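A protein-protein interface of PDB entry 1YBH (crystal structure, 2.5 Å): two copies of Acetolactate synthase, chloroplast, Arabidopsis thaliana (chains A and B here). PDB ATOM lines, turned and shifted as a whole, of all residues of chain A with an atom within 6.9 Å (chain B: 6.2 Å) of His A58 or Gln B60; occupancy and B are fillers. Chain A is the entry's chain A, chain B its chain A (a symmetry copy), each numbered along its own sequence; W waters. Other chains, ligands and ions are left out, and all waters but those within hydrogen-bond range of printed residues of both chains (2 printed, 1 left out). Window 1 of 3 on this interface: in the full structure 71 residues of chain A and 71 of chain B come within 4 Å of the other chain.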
ATOM      1  N   TYR A  33      24.668  16.274  20.263  1.00  0.00           N
ATOM      2  CA  TYR A  33      24.227  15.123  19.489  1.00  0.00           C
ATOM      3  C   TYR A  33      25.369  14.111  19.594  1.00  0.00           C
ATOM      4  O   TYR A  33      26.472  14.343  19.100  1.00  0.00           O
ATOM      5  CB  TYR A  33      24.006  15.532  18.036  1.00  0.00           C
ATOM      6  CG  TYR A  33      23.188  14.545  17.249  1.00  0.00           C
ATOM      7  CD1 TYR A  33      21.802  14.673  17.153  1.00  0.00           C
ATOM      8  CD2 TYR A  33      23.795  13.467  16.614  1.00  0.00           C
ATOM      9  CE1 TYR A  33      21.045  13.746  16.437  1.00  0.00           C
ATOM     10  CE2 TYR A  33      23.047  12.537  15.898  1.00  0.00           C
ATOM     11  CZ  TYR A  33      21.677  12.681  15.814  1.00  0.00           C
ATOM     12  OH  TYR A  33      20.946  11.751  15.115  1.00  0.00           O
ATOM     13  N   LEU A  55      18.895  17.457  23.000  1.00  0.00           N
ATOM     14  CA  LEU A  55      19.340  16.686  21.847  1.00  0.00           C
ATOM     15  C   LEU A  55      18.661  17.156  20.565  1.00  0.00           C
ATOM     16  O   LEU A  55      17.463  16.948  20.371  1.00  0.00           O
ATOM     17  CB  LEU A  55      19.029  15.207  22.069  1.00  0.00           C
ATOM     18  CG  LEU A  55      19.087  14.274  20.859  1.00  0.00           C
ATOM     19  CD1 LEU A  55      20.524  14.165  20.359  1.00  0.00           C
ATOM     20  CD2 LEU A  55      18.556  12.909  21.241  1.00  0.00           C
ATOM     21  N   PRO A  56      19.413  17.802  19.665  1.00  0.00           N
ATOM     22  CA  PRO A  56      18.805  18.267  18.414  1.00  0.00           C
ATOM     23  C   PRO A  56      18.692  17.085  17.454  1.00  0.00           C
ATOM     24  O   PRO A  56      19.061  15.965  17.808  1.00  0.00           O
ATOM     25  CB  PRO A  56      19.799  19.305  17.924  1.00  0.00           C
ATOM     26  CG  PRO A  56      21.107  18.680  18.318  1.00  0.00           C
ATOM     27  CD  PRO A  56      20.845  18.148  19.723  1.00  0.00           C
ATOM     28  N   ARG A  57      18.185  17.324  16.248  1.00  0.00           N
ATOM     29  CA  ARG A  57      18.073  16.254  15.264  1.00  0.00           C
ATOM     30  C   ARG A  57      19.140  16.386  14.181  1.00  0.00           C
ATOM     31  O   ARG A  57      19.275  15.523  13.311  1.00  0.00           O
ATOM     32  CB  ARG A  57      16.675  16.235  14.650  1.00  0.00           C
ATOM     33  CG  ARG A  57      15.774  15.193  15.288  1.00  0.00           C
ATOM     34  CD  ARG A  57      15.738  15.356  16.800  1.00  0.00           C
ATOM     35  NE  ARG A  57      14.930  14.328  17.450  1.00  0.00           N
ATOM     36  CZ  ARG A  57      14.749  14.252  18.765  1.00  0.00           C
ATOM     37  NH1 ARG A  57      15.321  15.147  19.559  1.00  0.00           N
ATOM     38  NH2 ARG A  57      13.998  13.289  19.286  1.00  0.00           N
ATOM     39  N   HIS A  58      19.899  17.471  14.259  1.00  0.00           N
ATOM     40  CA  HIS A  58      20.989  17.734  13.335  1.00  0.00           C
ATOM     41  C   HIS A  58      21.947  18.692  14.042  1.00  0.00           C
ATOM     42  O   HIS A  58      21.517  19.635  14.714  1.00  0.00           O
ATOM     43  CB  HIS A  58      20.469  18.368  12.051  1.00  0.00           C
ATOM     44  CG  HIS A  58      21.498  18.464  10.969  1.00  0.00           C
ATOM     45  ND1 HIS A  58      21.440  17.705   9.822  1.00  0.00           N
ATOM     46  CD2 HIS A  58      22.613  19.223  10.861  1.00  0.00           C
ATOM     47  CE1 HIS A  58      22.476  17.989   9.052  1.00  0.00           C
ATOM     48  NE2 HIS A  58      23.205  18.907   9.662  1.00  0.00           N
ATOM     49  N   GLU A  59      23.242  18.435  13.888  1.00  0.00           N
ATOM     50  CA  GLU A  59      24.295  19.237  14.515  1.00  0.00           C
ATOM     51  C   GLU A  59      24.140  20.723  14.211  1.00  0.00           C
ATOM     52  O   GLU A  59      24.479  21.569  15.042  1.00  0.00           O
ATOM     53  CB  GLU A  59      25.653  18.757  14.029  1.00  0.00           C
ATOM     54  CG  GLU A  59      25.589  17.382  13.374  1.00  0.00           C
ATOM     55  CD  GLU A  59      25.897  16.300  14.348  1.00  0.00           C
ATOM     56  OE1 GLU A  59      25.845  15.114  13.974  1.00  0.00           O
ATOM     57  OE2 GLU A  59      26.204  16.654  15.501  1.00  0.00           O
ATOM     58  N   GLN A  60      23.647  21.044  13.016  1.00  0.00           N
ATOM     59  CA  GLN A  60      23.450  22.437  12.649  1.00  0.00           C
ATOM     60  C   GLN A  60      22.324  23.008  13.509  1.00  0.00           C
ATOM     61  O   GLN A  60      22.306  24.201  13.821  1.00  0.00           O
ATOM     62  CB  GLN A  60      23.115  22.575  11.163  1.00  0.00           C
ATOM     63  CG  GLN A  60      22.756  23.993  10.777  1.00  0.00           C
ATOM     64  CD  GLN A  60      22.830  24.240   9.287  1.00  0.00           C
ATOM     65  OE1 GLN A  60      23.916  24.242   8.700  1.00  0.00           O
ATOM     66  NE2 GLN A  60      21.677  24.454   8.664  1.00  0.00           N
ATOM     67  N   GLY A  61      21.376  22.149  13.877  1.00  0.00           N
ATOM     68  CA  GLY A  61      20.288  22.574  14.742  1.00  0.00           C
ATOM     69  C   GLY A  61      20.918  22.867  16.093  1.00  0.00           C
ATOM     70  O   GLY A  61      20.557  23.836  16.765  1.00  0.00           O
ATOM     71  N   GLY A  62      21.882  22.031  16.479  1.00  0.00           N
ATOM     72  CA  GLY A  62      22.584  22.212  17.737  1.00  0.00           C
ATOM     73  C   GLY A  62      23.250  23.572  17.848  1.00  0.00           C
ATOM     74  O   GLY A  62      22.985  24.308  18.797  1.00  0.00           O
ATOM     75  N   VAL A  63      24.109  23.922  16.884  1.00  0.00           N
ATOM     76  CA  VAL A  63      24.786  25.218  16.919  1.00  0.00           C
ATOM     77  C   VAL A  63      23.818  26.385  16.908  1.00  0.00           C
ATOM     78  O   VAL A  63      23.920  27.292  17.738  1.00  0.00           O
ATOM     79  CB  VAL A  63      25.724  25.460  15.713  1.00  0.00           C
ATOM     80  CG1 VAL A  63      27.157  25.488  16.184  1.00  0.00           C
ATOM     81  CG2 VAL A  63      25.489  24.430  14.634  1.00  0.00           C
ATOM     82  N   PRO A  85      31.947  14.049  10.572  1.00  0.00           N
ATOM     83  CA  PRO A  85      30.682  14.612  10.093  1.00  0.00           C
ATOM     84  C   PRO A  85      29.964  15.414  11.164  1.00  0.00           C
ATOM     85  O   PRO A  85      29.243  16.360  10.857  1.00  0.00           O
ATOM     86  CB  PRO A  85      29.895  13.380   9.650  1.00  0.00           C
ATOM     87  CG  PRO A  85      30.348  12.343  10.611  1.00  0.00           C
ATOM     88  CD  PRO A  85      31.857  12.583  10.676  1.00  0.00           C
ATOM     89  N   THR A  88      32.013  18.803  11.132  1.00  0.00           N
ATOM     90  CA  THR A  88      31.800  19.601   9.932  1.00  0.00           C
ATOM     91  C   THR A  88      30.387  20.170   9.872  1.00  0.00           C
ATOM     92  O   THR A  88      30.169  21.223   9.281  1.00  0.00           O
ATOM     93  CB  THR A  88      32.081  18.800   8.636  1.00  0.00           C
ATOM     94  OG1 THR A  88      31.217  17.659   8.567  1.00  0.00           O
ATOM     95  CG2 THR A  88      33.537  18.347   8.608  1.00  0.00           C
ATOM     96  N   ASN A  89      29.429  19.488  10.486  1.00  0.00           N
ATOM     97  CA  ASN A  89      28.054  19.977  10.477  1.00  0.00           C
ATOM     98  C   ASN A  89      27.864  21.231  11.338  1.00  0.00           C
ATOM     99  O   ASN A  89      26.794  21.838  11.336  1.00  0.00           O
ATOM    100  CB  ASN A  89      27.098  18.885  10.947  1.00  0.00           C
ATOM    101  CG  ASN A  89      26.626  17.992   9.813  1.00  0.00           C
ATOM    102  OD1 ASN A  89      26.000  16.965  10.053  1.00  0.00           O
ATOM    103  ND2 ASN A  89      26.906  18.384   8.579  1.00  0.00           N
ATOM    104  N   LEU A  90      28.904  21.619  12.069  1.00  0.00           N
ATOM    105  CA  LEU A  90      28.838  22.808  12.916  1.00  0.00           C
ATOM    106  C   LEU A  90      29.277  24.054  12.166  1.00  0.00           C
ATOM    107  O   LEU A  90      28.862  25.161  12.498  1.00  0.00           O
ATOM    108  CB  LEU A  90      29.756  22.660  14.121  1.00  0.00           C
ATOM    109  CG  LEU A  90      29.493  21.589  15.166  1.00  0.00           C
ATOM    110  CD1 LEU A  90      30.633  21.594  16.163  1.00  0.00           C
ATOM    111  CD2 LEU A  90      28.186  21.872  15.865  1.00  0.00           C
ATOM    112  N   MET A 458      14.518  23.908   5.754  1.00  0.00           N
ATOM    113  CA  MET A 458      15.916  23.501   5.870  1.00  0.00           C
ATOM    114  C   MET A 458      16.233  22.758   7.156  1.00  0.00           C
ATOM    115  O   MET A 458      16.968  21.776   7.130  1.00  0.00           O
ATOM    116  CB  MET A 458      16.851  24.698   5.733  1.00  0.00           C
ATOM    117  CG  MET A 458      16.920  25.252   4.339  1.00  0.00           C
ATOM    118  SD  MET A 458      18.238  26.453   4.164  1.00  0.00           S
ATOM    119  CE  MET A 458      18.966  25.925   2.612  1.00  0.00           C
ATOM    120  N   ASN A 459      15.707  23.225   8.280  1.00  0.00           N
ATOM    121  CA  ASN A 459      15.950  22.538   9.547  1.00  0.00           C
ATOM    122  C   ASN A 459      14.641  22.138  10.195  1.00  0.00           C
ATOM    123  O   ASN A 459      14.478  22.192  11.414  1.00  0.00           O
ATOM    124  CB  ASN A 459      16.781  23.411  10.485  1.00  0.00           C
ATOM    125  CG  ASN A 459      18.239  23.440  10.089  1.00  0.00           C
ATOM    126  OD1 ASN A 459      18.844  22.391   9.856  1.00  0.00           O
ATOM    127  ND2 ASN A 459      18.812  24.636   9.999  1.00  0.00           N
ATOM    128  N   GLN A 461      13.535  19.362  10.706  1.00  0.00           N
ATOM    129  CA  GLN A 461      13.666  18.231  11.614  1.00  0.00           C
ATOM    130  C   GLN A 461      13.694  18.656  13.074  1.00  0.00           C
ATOM    131  O   GLN A 461      13.461  17.843  13.965  1.00  0.00           O
ATOM    132  CB  GLN A 461      14.921  17.407  11.302  1.00  0.00           C
ATOM    133  CG  GLN A 461      16.239  17.970  11.820  1.00  0.00           C
ATOM    134  CD  GLN A 461      16.709  19.183  11.050  1.00  0.00           C
ATOM    135  OE1 GLN A 461      16.347  19.376   9.889  1.00  0.00           O
ATOM    136  NE2 GLN A 461      17.538  20.007  11.688  1.00  0.00           N
ATOM    137  N   GLU A 462      13.973  19.922  13.337  1.00  0.00           N
ATOM    138  CA  GLU A 462      14.011  20.356  14.719  1.00  0.00           C
ATOM    139  C   GLU A 462      12.623  20.417  15.361  1.00  0.00           C
ATOM    140  O   GLU A 462      12.503  20.637  16.567  1.00  0.00           O
ATOM    141  CB  GLU A 462      14.725  21.704  14.832  1.00  0.00           C
ATOM    142  CG  GLU A 462      16.205  21.645  14.440  1.00  0.00           C
ATOM    143  CD  GLU A 462      16.958  20.453  15.055  1.00  0.00           C
ATOM    144  OE1 GLU A 462      16.756  20.153  16.254  1.00  0.00           O
ATOM    145  OE2 GLU A 462      17.764  19.820  14.337  1.00  0.00           O
ATOM    146  N   THR A 465      12.535  18.028  17.969  1.00  0.00           N
ATOM    147  CA  THR A 465      13.207  18.501  19.178  1.00  0.00           C
ATOM    148  C   THR A 465      12.237  19.303  20.046  1.00  0.00           C
ATOM    149  O   THR A 465      12.119  19.071  21.256  1.00  0.00           O
ATOM    150  CB  THR A 465      14.404  19.403  18.814  1.00  0.00           C
ATOM    151  OG1 THR A 465      15.362  18.644  18.068  1.00  0.00           O
ATOM    152  CG2 THR A 465      15.062  19.959  20.063  1.00  0.00           C
ATOM    153  N   HIS B  58      18.270  21.986   0.665  1.00  0.00           N
ATOM    154  CA  HIS B  58      19.380  22.344   1.531  1.00  0.00           C
ATOM    155  C   HIS B  58      20.661  22.018   0.766  1.00  0.00           C
ATOM    156  O   HIS B  58      20.756  20.980   0.104  1.00  0.00           O
ATOM    157  CB  HIS B  58      19.330  21.549   2.831  1.00  0.00           C
ATOM    158  CG  HIS B  58      20.309  22.020   3.860  1.00  0.00           C
ATOM    159  ND1 HIS B  58      19.919  22.653   5.019  1.00  0.00           N
ATOM    160  CD2 HIS B  58      21.660  21.956   3.904  1.00  0.00           C
ATOM    161  CE1 HIS B  58      20.987  22.962   5.734  1.00  0.00           C
ATOM    162  NE2 HIS B  58      22.057  22.551   5.077  1.00  0.00           N
ATOM    163  N   GLU B  59      21.637  22.915   0.861  1.00  0.00           N
ATOM    164  CA  GLU B  59      22.922  22.773   0.173  1.00  0.00           C
ATOM    165  C   GLU B  59      23.582  21.429   0.464  1.00  0.00           C
ATOM    166  O   GLU B  59      24.272  20.874  -0.394  1.00  0.00           O
ATOM    167  CB  GLU B  59      23.852  23.899   0.599  1.00  0.00           C
ATOM    168  CG  GLU B  59      23.110  25.046   1.275  1.00  0.00           C
ATOM    169  CD  GLU B  59      22.760  26.117   0.301  1.00  0.00           C
ATOM    170  OE1 GLU B  59      22.114  27.106   0.694  1.00  0.00           O
ATOM    171  OE2 GLU B  59      23.151  25.959  -0.869  1.00  0.00           O
ATOM    172  N   GLN B  60      23.387  20.915   1.677  1.00  0.00           N
ATOM    173  CA  GLN B  60      23.964  19.629   2.033  1.00  0.00           C
ATOM    174  C   GLN B  60      23.263  18.543   1.221  1.00  0.00           C
ATOM    175  O   GLN B  60      23.856  17.511   0.894  1.00  0.00           O
ATOM    176  CB  GLN B  60      23.824  19.357   3.531  1.00  0.00           C
ATOM    177  CG  GLN B  60      24.277  17.966   3.915  1.00  0.00           C
ATOM    178  CD  GLN B  60      24.541  17.814   5.396  1.00  0.00           C
ATOM    179  OE1 GLN B  60      25.496  18.388   5.931  1.00  0.00           O
ATOM    180  NE2 GLN B  60      23.702  17.038   6.072  1.00  0.00           N
ATOM    181  N   GLY B  61      21.989  18.774   0.911  1.00  0.00           N
ATOM    182  CA  GLY B  61      21.243  17.832   0.094  1.00  0.00           C
ATOM    183  C   GLY B  61      21.866  17.892  -1.290  1.00  0.00           C
ATOM    184  O   GLY B  61      22.033  16.869  -1.956  1.00  0.00           O
ATOM    185  N   GLY B  62      22.232  19.104  -1.710  1.00  0.00           N
ATOM    186  CA  GLY B  62      22.863  19.300  -3.004  1.00  0.00           C
ATOM    187  C   GLY B  62      24.135  18.486  -3.165  1.00  0.00           C
ATOM    188  O   GLY B  62      24.248  17.706  -4.110  1.00  0.00           O
ATOM    189  N   VAL B  63      25.096  18.650  -2.249  1.00  0.00           N
ATOM    190  CA  VAL B  63      26.348  17.897  -2.333  1.00  0.00           C
ATOM    191  C   VAL B  63      26.134  16.397  -2.292  1.00  0.00           C
ATOM    192  O   VAL B  63      26.655  15.666  -3.138  1.00  0.00           O
ATOM    193  CB  VAL B  63      27.331  18.198  -1.178  1.00  0.00           C
ATOM    194  CG1 VAL B  63      28.542  18.916  -1.719  1.00  0.00           C
ATOM    195  CG2 VAL B  63      26.646  18.968  -0.076  1.00  0.00           C
ATOM    196  N   PHE B  64      25.397  15.934  -1.285  1.00  0.00           N
ATOM    197  CA  PHE B  64      25.128  14.509  -1.145  1.00  0.00           C
ATOM    198  C   PHE B  64      24.454  13.956  -2.402  1.00  0.00           C
ATOM    199  O   PHE B  64      24.755  12.838  -2.821  1.00  0.00           O
ATOM    200  CB  PHE B  64      24.275  14.248   0.099  1.00  0.00           C
ATOM    201  CG  PHE B  64      25.036  14.348   1.396  1.00  0.00           C
ATOM    202  CD1 PHE B  64      24.354  14.421   2.606  1.00  0.00           C
ATOM    203  CD2 PHE B  64      26.427  14.341   1.414  1.00  0.00           C
ATOM    204  CE1 PHE B  64      25.045  14.489   3.819  1.00  0.00           C
ATOM    205  CE2 PHE B  64      27.129  14.408   2.617  1.00  0.00           C
ATOM    206  CZ  PHE B  64      26.436  14.484   3.824  1.00  0.00           C
ATOM    207  N   ALA B  65      23.558  14.729  -3.013  1.00  0.00           N
ATOM    208  CA  ALA B  65      22.910  14.278  -4.248  1.00  0.00           C
ATOM    209  C   ALA B  65      23.982  14.155  -5.342  1.00  0.00           C
ATOM    210  O   ALA B  65      24.028  13.169  -6.090  1.00  0.00           O
ATOM    211  CB  ALA B  65      21.837  15.267  -4.673  1.00  0.00           C
ATOM    212  N   ASN B  89      27.618  25.296   3.944  1.00  0.00           N
ATOM    213  CA  ASN B  89      26.704  24.160   4.013  1.00  0.00           C
ATOM    214  C   ASN B  89      27.156  22.981   3.146  1.00  0.00           C
ATOM    215  O   ASN B  89      26.562  21.904   3.191  1.00  0.00           O
ATOM    216  CB  ASN B  89      25.297  24.586   3.605  1.00  0.00           C
ATOM    217  CG  ASN B  89      24.484  25.117   4.773  1.00  0.00           C
ATOM    218  OD1 ASN B  89      23.403  25.662   4.578  1.00  0.00           O
ATOM    219  ND2 ASN B  89      24.987  24.945   5.987  1.00  0.00           N
ATOM    220  N   LEU B  90      28.210  23.183   2.360  1.00  0.00           N
ATOM    221  CA  LEU B  90      28.732  22.124   1.501  1.00  0.00           C
ATOM    222  C   LEU B  90      29.793  21.300   2.211  1.00  0.00           C
ATOM    223  O   LEU B  90      30.003  20.135   1.885  1.00  0.00           O
ATOM    224  CB  LEU B  90      29.378  22.713   0.255  1.00  0.00           C
ATOM    225  CG  LEU B  90      28.545  23.474  -0.761  1.00  0.00           C
ATOM    226  CD1 LEU B  90      29.469  24.052  -1.812  1.00  0.00           C
ATOM    227  CD2 LEU B  90      27.546  22.540  -1.399  1.00  0.00           C
ATOM    228  N   SER B  92      30.462  19.302   4.853  1.00  0.00           N
ATOM    229  CA  SER B  92      30.370  17.865   5.131  1.00  0.00           C
ATOM    230  C   SER B  92      30.417  17.030   3.854  1.00  0.00           C
ATOM    231  O   SER B  92      31.000  15.951   3.840  1.00  0.00           O
ATOM    232  CB  SER B  92      29.094  17.537   5.902  1.00  0.00           C
ATOM    233  OG  SER B  92      29.114  18.151   7.173  1.00  0.00           O
ATOM    234  N   GLY B  93      29.798  17.529   2.787  1.00  0.00           N
ATOM    235  CA  GLY B  93      29.806  16.806   1.528  1.00  0.00           C
ATOM    236  C   GLY B  93      31.207  16.739   0.941  1.00  0.00           C
ATOM    237  O   GLY B  93      31.641  15.694   0.461  1.00  0.00           O
ATOM    238  N   MET B 428      25.776  10.924   8.528  1.00  0.00           N
ATOM    239  CA  MET B 428      24.347  10.642   8.574  1.00  0.00           C
ATOM    240  C   MET B 428      23.614  11.622   7.653  1.00  0.00           C
ATOM    241  O   MET B 428      24.120  12.710   7.369  1.00  0.00           O
ATOM    242  CB  MET B 428      23.827  10.800  10.004  1.00  0.00           C
ATOM    243  CG  MET B 428      24.149   9.636  10.916  1.00  0.00           C
ATOM    244  SD  MET B 428      23.712  10.012  12.613  1.00  0.00           S
ATOM    245  CE  MET B 428      21.919  10.014  12.530  1.00  0.00           C
ATOM    246  N   GLY B 429      22.427  11.239   7.188  1.00  0.00           N
ATOM    247  CA  GLY B 429      21.659  12.112   6.316  1.00  0.00           C
ATOM    248  C   GLY B 429      22.081  12.029   4.864  1.00  0.00           C
ATOM    249  O   GLY B 429      21.591  12.779   4.022  1.00  0.00           O
ATOM    250  N   PHE B 430      22.981  11.098   4.576  1.00  0.00           N
ATOM    251  CA  PHE B 430      23.510  10.888   3.234  1.00  0.00           C
ATOM    252  C   PHE B 430      22.569  10.088   2.320  1.00  0.00           C
ATOM    253  O   PHE B 430      22.436  10.380   1.125  1.00  0.00           O
ATOM    254  CB  PHE B 430      24.848  10.153   3.352  1.00  0.00           C
ATOM    255  CG  PHE B 430      25.446   9.736   2.040  1.00  0.00           C
ATOM    256  CD1 PHE B 430      26.229  10.616   1.303  1.00  0.00           C
ATOM    257  CD2 PHE B 430      25.248   8.448   1.554  1.00  0.00           C
ATOM    258  CE1 PHE B 430      26.816  10.218   0.102  1.00  0.00           C
ATOM    259  CE2 PHE B 430      25.830   8.042   0.355  1.00  0.00           C
ATOM    260  CZ  PHE B 430      26.617   8.929  -0.371  1.00  0.00           C
ATOM    261  N   PRO B 433      19.482  11.995   0.063  1.00  0.00           N
ATOM    262  CA  PRO B 433      20.016  12.830  -1.020  1.00  0.00           C
ATOM    263  C   PRO B 433      20.798  11.996  -2.042  1.00  0.00           C
ATOM    264  O   PRO B 433      20.709  12.235  -3.244  1.00  0.00           O
ATOM    265  CB  PRO B 433      20.916  13.818  -0.285  1.00  0.00           C
ATOM    266  CG  PRO B 433      20.333  13.863   1.094  1.00  0.00           C
ATOM    267  CD  PRO B 433      19.994  12.440   1.370  1.00  0.00           C
ATOM    268  N   MET B 458      17.462  13.803   9.332  1.00  0.00           N
ATOM    269  CA  MET B 458      18.434  14.879   9.154  1.00  0.00           C
ATOM    270  C   MET B 458      18.253  15.660   7.865  1.00  0.00           C
ATOM    271  O   MET B 458      18.369  16.883   7.869  1.00  0.00           O
ATOM    272  CB  MET B 458      19.863  14.349   9.230  1.00  0.00           C
ATOM    273  CG  MET B 458      20.278  13.931  10.610  1.00  0.00           C
ATOM    274  SD  MET B 458      22.036  13.598  10.706  1.00  0.00           S
ATOM    275  CE  MET B 458      22.455  14.450  12.227  1.00  0.00           C
ATOM    276  N   ASN B 459      17.996  14.972   6.761  1.00  0.00           N
ATOM    277  CA  ASN B 459      17.784  15.668   5.493  1.00  0.00           C
ATOM    278  C   ASN B 459      16.427  15.316   4.915  1.00  0.00           C
ATOM    279  O   ASN B 459      16.258  15.169   3.705  1.00  0.00           O
ATOM    280  CB  ASN B 459      18.900  15.344   4.504  1.00  0.00           C
ATOM    281  CG  ASN B 459      20.175  16.087   4.829  1.00  0.00           C
ATOM    282  OD1 ASN B 459      20.155  17.300   5.046  1.00  0.00           O
ATOM    283  ND2 ASN B 459      21.293  15.368   4.875  1.00  0.00           N
ATOM    284  N   GLN B 461      14.012  17.098   4.496  1.00  0.00           N
ATOM    285  CA  GLN B 461      13.488  18.119   3.598  1.00  0.00           C
ATOM    286  C   GLN B 461      13.663  17.751   2.132  1.00  0.00           C
ATOM    287  O   GLN B 461      12.997  18.311   1.266  1.00  0.00           O
ATOM    288  CB  GLN B 461      14.141  19.481   3.860  1.00  0.00           C
ATOM    289  CG  GLN B 461      15.532  19.682   3.271  1.00  0.00           C
ATOM    290  CD  GLN B 461      16.604  18.904   4.001  1.00  0.00           C
ATOM    291  OE1 GLN B 461      16.452  18.567   5.176  1.00  0.00           O
ATOM    292  NE2 GLN B 461      17.708  18.626   3.313  1.00  0.00           N
ATOM    293  N   GLU B 462      14.549  16.813   1.839  1.00  0.00           N
ATOM    294  CA  GLU B 462      14.741  16.444   0.452  1.00  0.00           C
ATOM    295  C   GLU B 462      13.560  15.658  -0.123  1.00  0.00           C
ATOM    296  O   GLU B 462      13.515  15.392  -1.325  1.00  0.00           O
ATOM    297  CB  GLU B 462      16.048  15.667   0.286  1.00  0.00           C
ATOM    298  CG  GLU B 462      17.296  16.496   0.607  1.00  0.00           C
ATOM    299  CD  GLU B 462      17.285  17.897  -0.028  1.00  0.00           C
ATOM    300  OE1 GLU B 462      16.897  18.031  -1.211  1.00  0.00           O
ATOM    301  OE2 GLU B 462      17.675  18.867   0.659  1.00  0.00           O
HETATM  302  O   HOH W   1      24.851  15.328   7.833  1.00  0.00           O
HETATM  303  O   HOH W   2      21.677  26.488   6.873  1.00  0.00           O
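The side-chain amide nitrogen of Asn A459 lies close to the side-chain amide nitrogen of Gln A60, 3.2 Å away.
The side-chain amide nitrogen (NE2) of Gln B461 is in hydrogen-bond range of the side-chain carboxylate (OE2) of Glu B462, 2.7 Å away.
The backbone carbonyl oxygen (O) of Leu A55 is in hydrogen-bond range of the guanidinium group (NH1) of Arg A57, 2.9 Å away.
The side-chain amide oxygen of Asn B459 is in hydrogen-bond range of the side-chain amide nitrogen of Gln B461, 3.3 Å away.
The side-chain carboxylate of Glu A462 is in hydrogen-bond range of the side-chain amide nitrogen of Gln A461, at 2.7 Å.
NE2 of His A58 is in hydrogen-bond range of OD1 of Asn A89, 3.4 Å away.
His A58 touches two residues of chain B.
Gln B60 touches two residues of chain A.
Of the printed residues of chain B, Glu A59 touches Met B458.
Printed residues of chain A within 4 Å of Met B428: Tyr A33 (3.3 Å).
Leu A90 touches none of the printed residues of chain B.
The nearest residue of chain B that does not touch His A58 is Asn B459 (4.7 Å).
The side-chain amide nitrogen (ND2) of Asn A89 is in hydrogen-bond range of the side-chain amide oxygen (OE1) of Gln B60, at 3.0 Å.
The side-chain amide nitrogen of Asn B89 lies within hydrogen-bond range of the side-chain amide oxygen of Gln A60, at 3.0 Å.
OG1 of Thr A88 lies within hydrogen-bond range of OG of Ser B92.
The side-chain amide nitrogen (ND2) of Asn A89 is in hydrogen-bond range of the side-chain hydroxyl (OG) of Ser B92 (2.6 Å).
His A58 touches Gln B60, and with the chains exchanged Gln A60 touches His B58.
His A58 touches Met B458, and with the chains exchanged Met A458 touches His B58.
Glu A59 touches Met B458, and with the chains exchanged Met A458 touches Glu B59.
Gln A60 touches Asn B89, and with the chains exchanged Asn A89 touches Gln B60.
Positions printed for both chains: 58, 59, 60, 61, 62, 63, 89, 90, 458, 459, 461 and 462.
Of the 14 pairs that touch across the chains among the printed residues, 10 have their exchanged pair printed and touching as well.
Water W1 lies within hydrogen-bond range of NE2 of Gln B60 (2.7 Å), O of Met B428 (2.8 Å) and OD1 of Asn A89 (3.0 Å).
Water W2 lies within hydrogen-bond range of NE2 of Gln A60 (2.7 Å) and OD1 of Asn B89 (3.0 Å).
Of the 19 printed residues of chain A, 9 touch a printed residue of chain B.
Printed residues of chain A that touch a printed residue of chain B: Tyr A33, Arg A57, His A58, Glu A59, Gln A60, Thr A88, Asn A89, Met A458 and Gln A461.
Hydrophobic or aromatic side chains of chain A that line the printed part of chain B: Tyr A33, His A58 and Met A458.
Of the 20 printed residues of chain B, 8 touch a printed residue of chain A.
Hydrophobic or aromatic side chains of chain B that line the printed part of chain A: His B58, Met B428 and Met B458.
Along chain B the printed residues that touch a printed residue of chain A span positions 58 to 461.
Among the printed residues, 14 pairs touch across the chains.
Among the printed residues, no Asp or Glu carboxylate lies within 4 Å of a Lys or Arg side-chain nitrogen of the other chain.
Among the printed residues, merely in contact across the chains: Tyr A33 with Met B428 (3.3 Å), Arg A57 with Met B458 (3.3 Å), His A58 with Gln B60 (3.4 Å), His A58 with Met B458 (3.7 Å), Glu A59 with Met B458 (3.9 Å), Gln A60 with His B58 (3.4 Å), Met A458 with His B58 (3.7 Å), Met A458 with Glu B59 (3.9 Å), Met A458 with Gln B461 (3.8 Å) and Gln A461 with Met B458 (3.8 Å).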
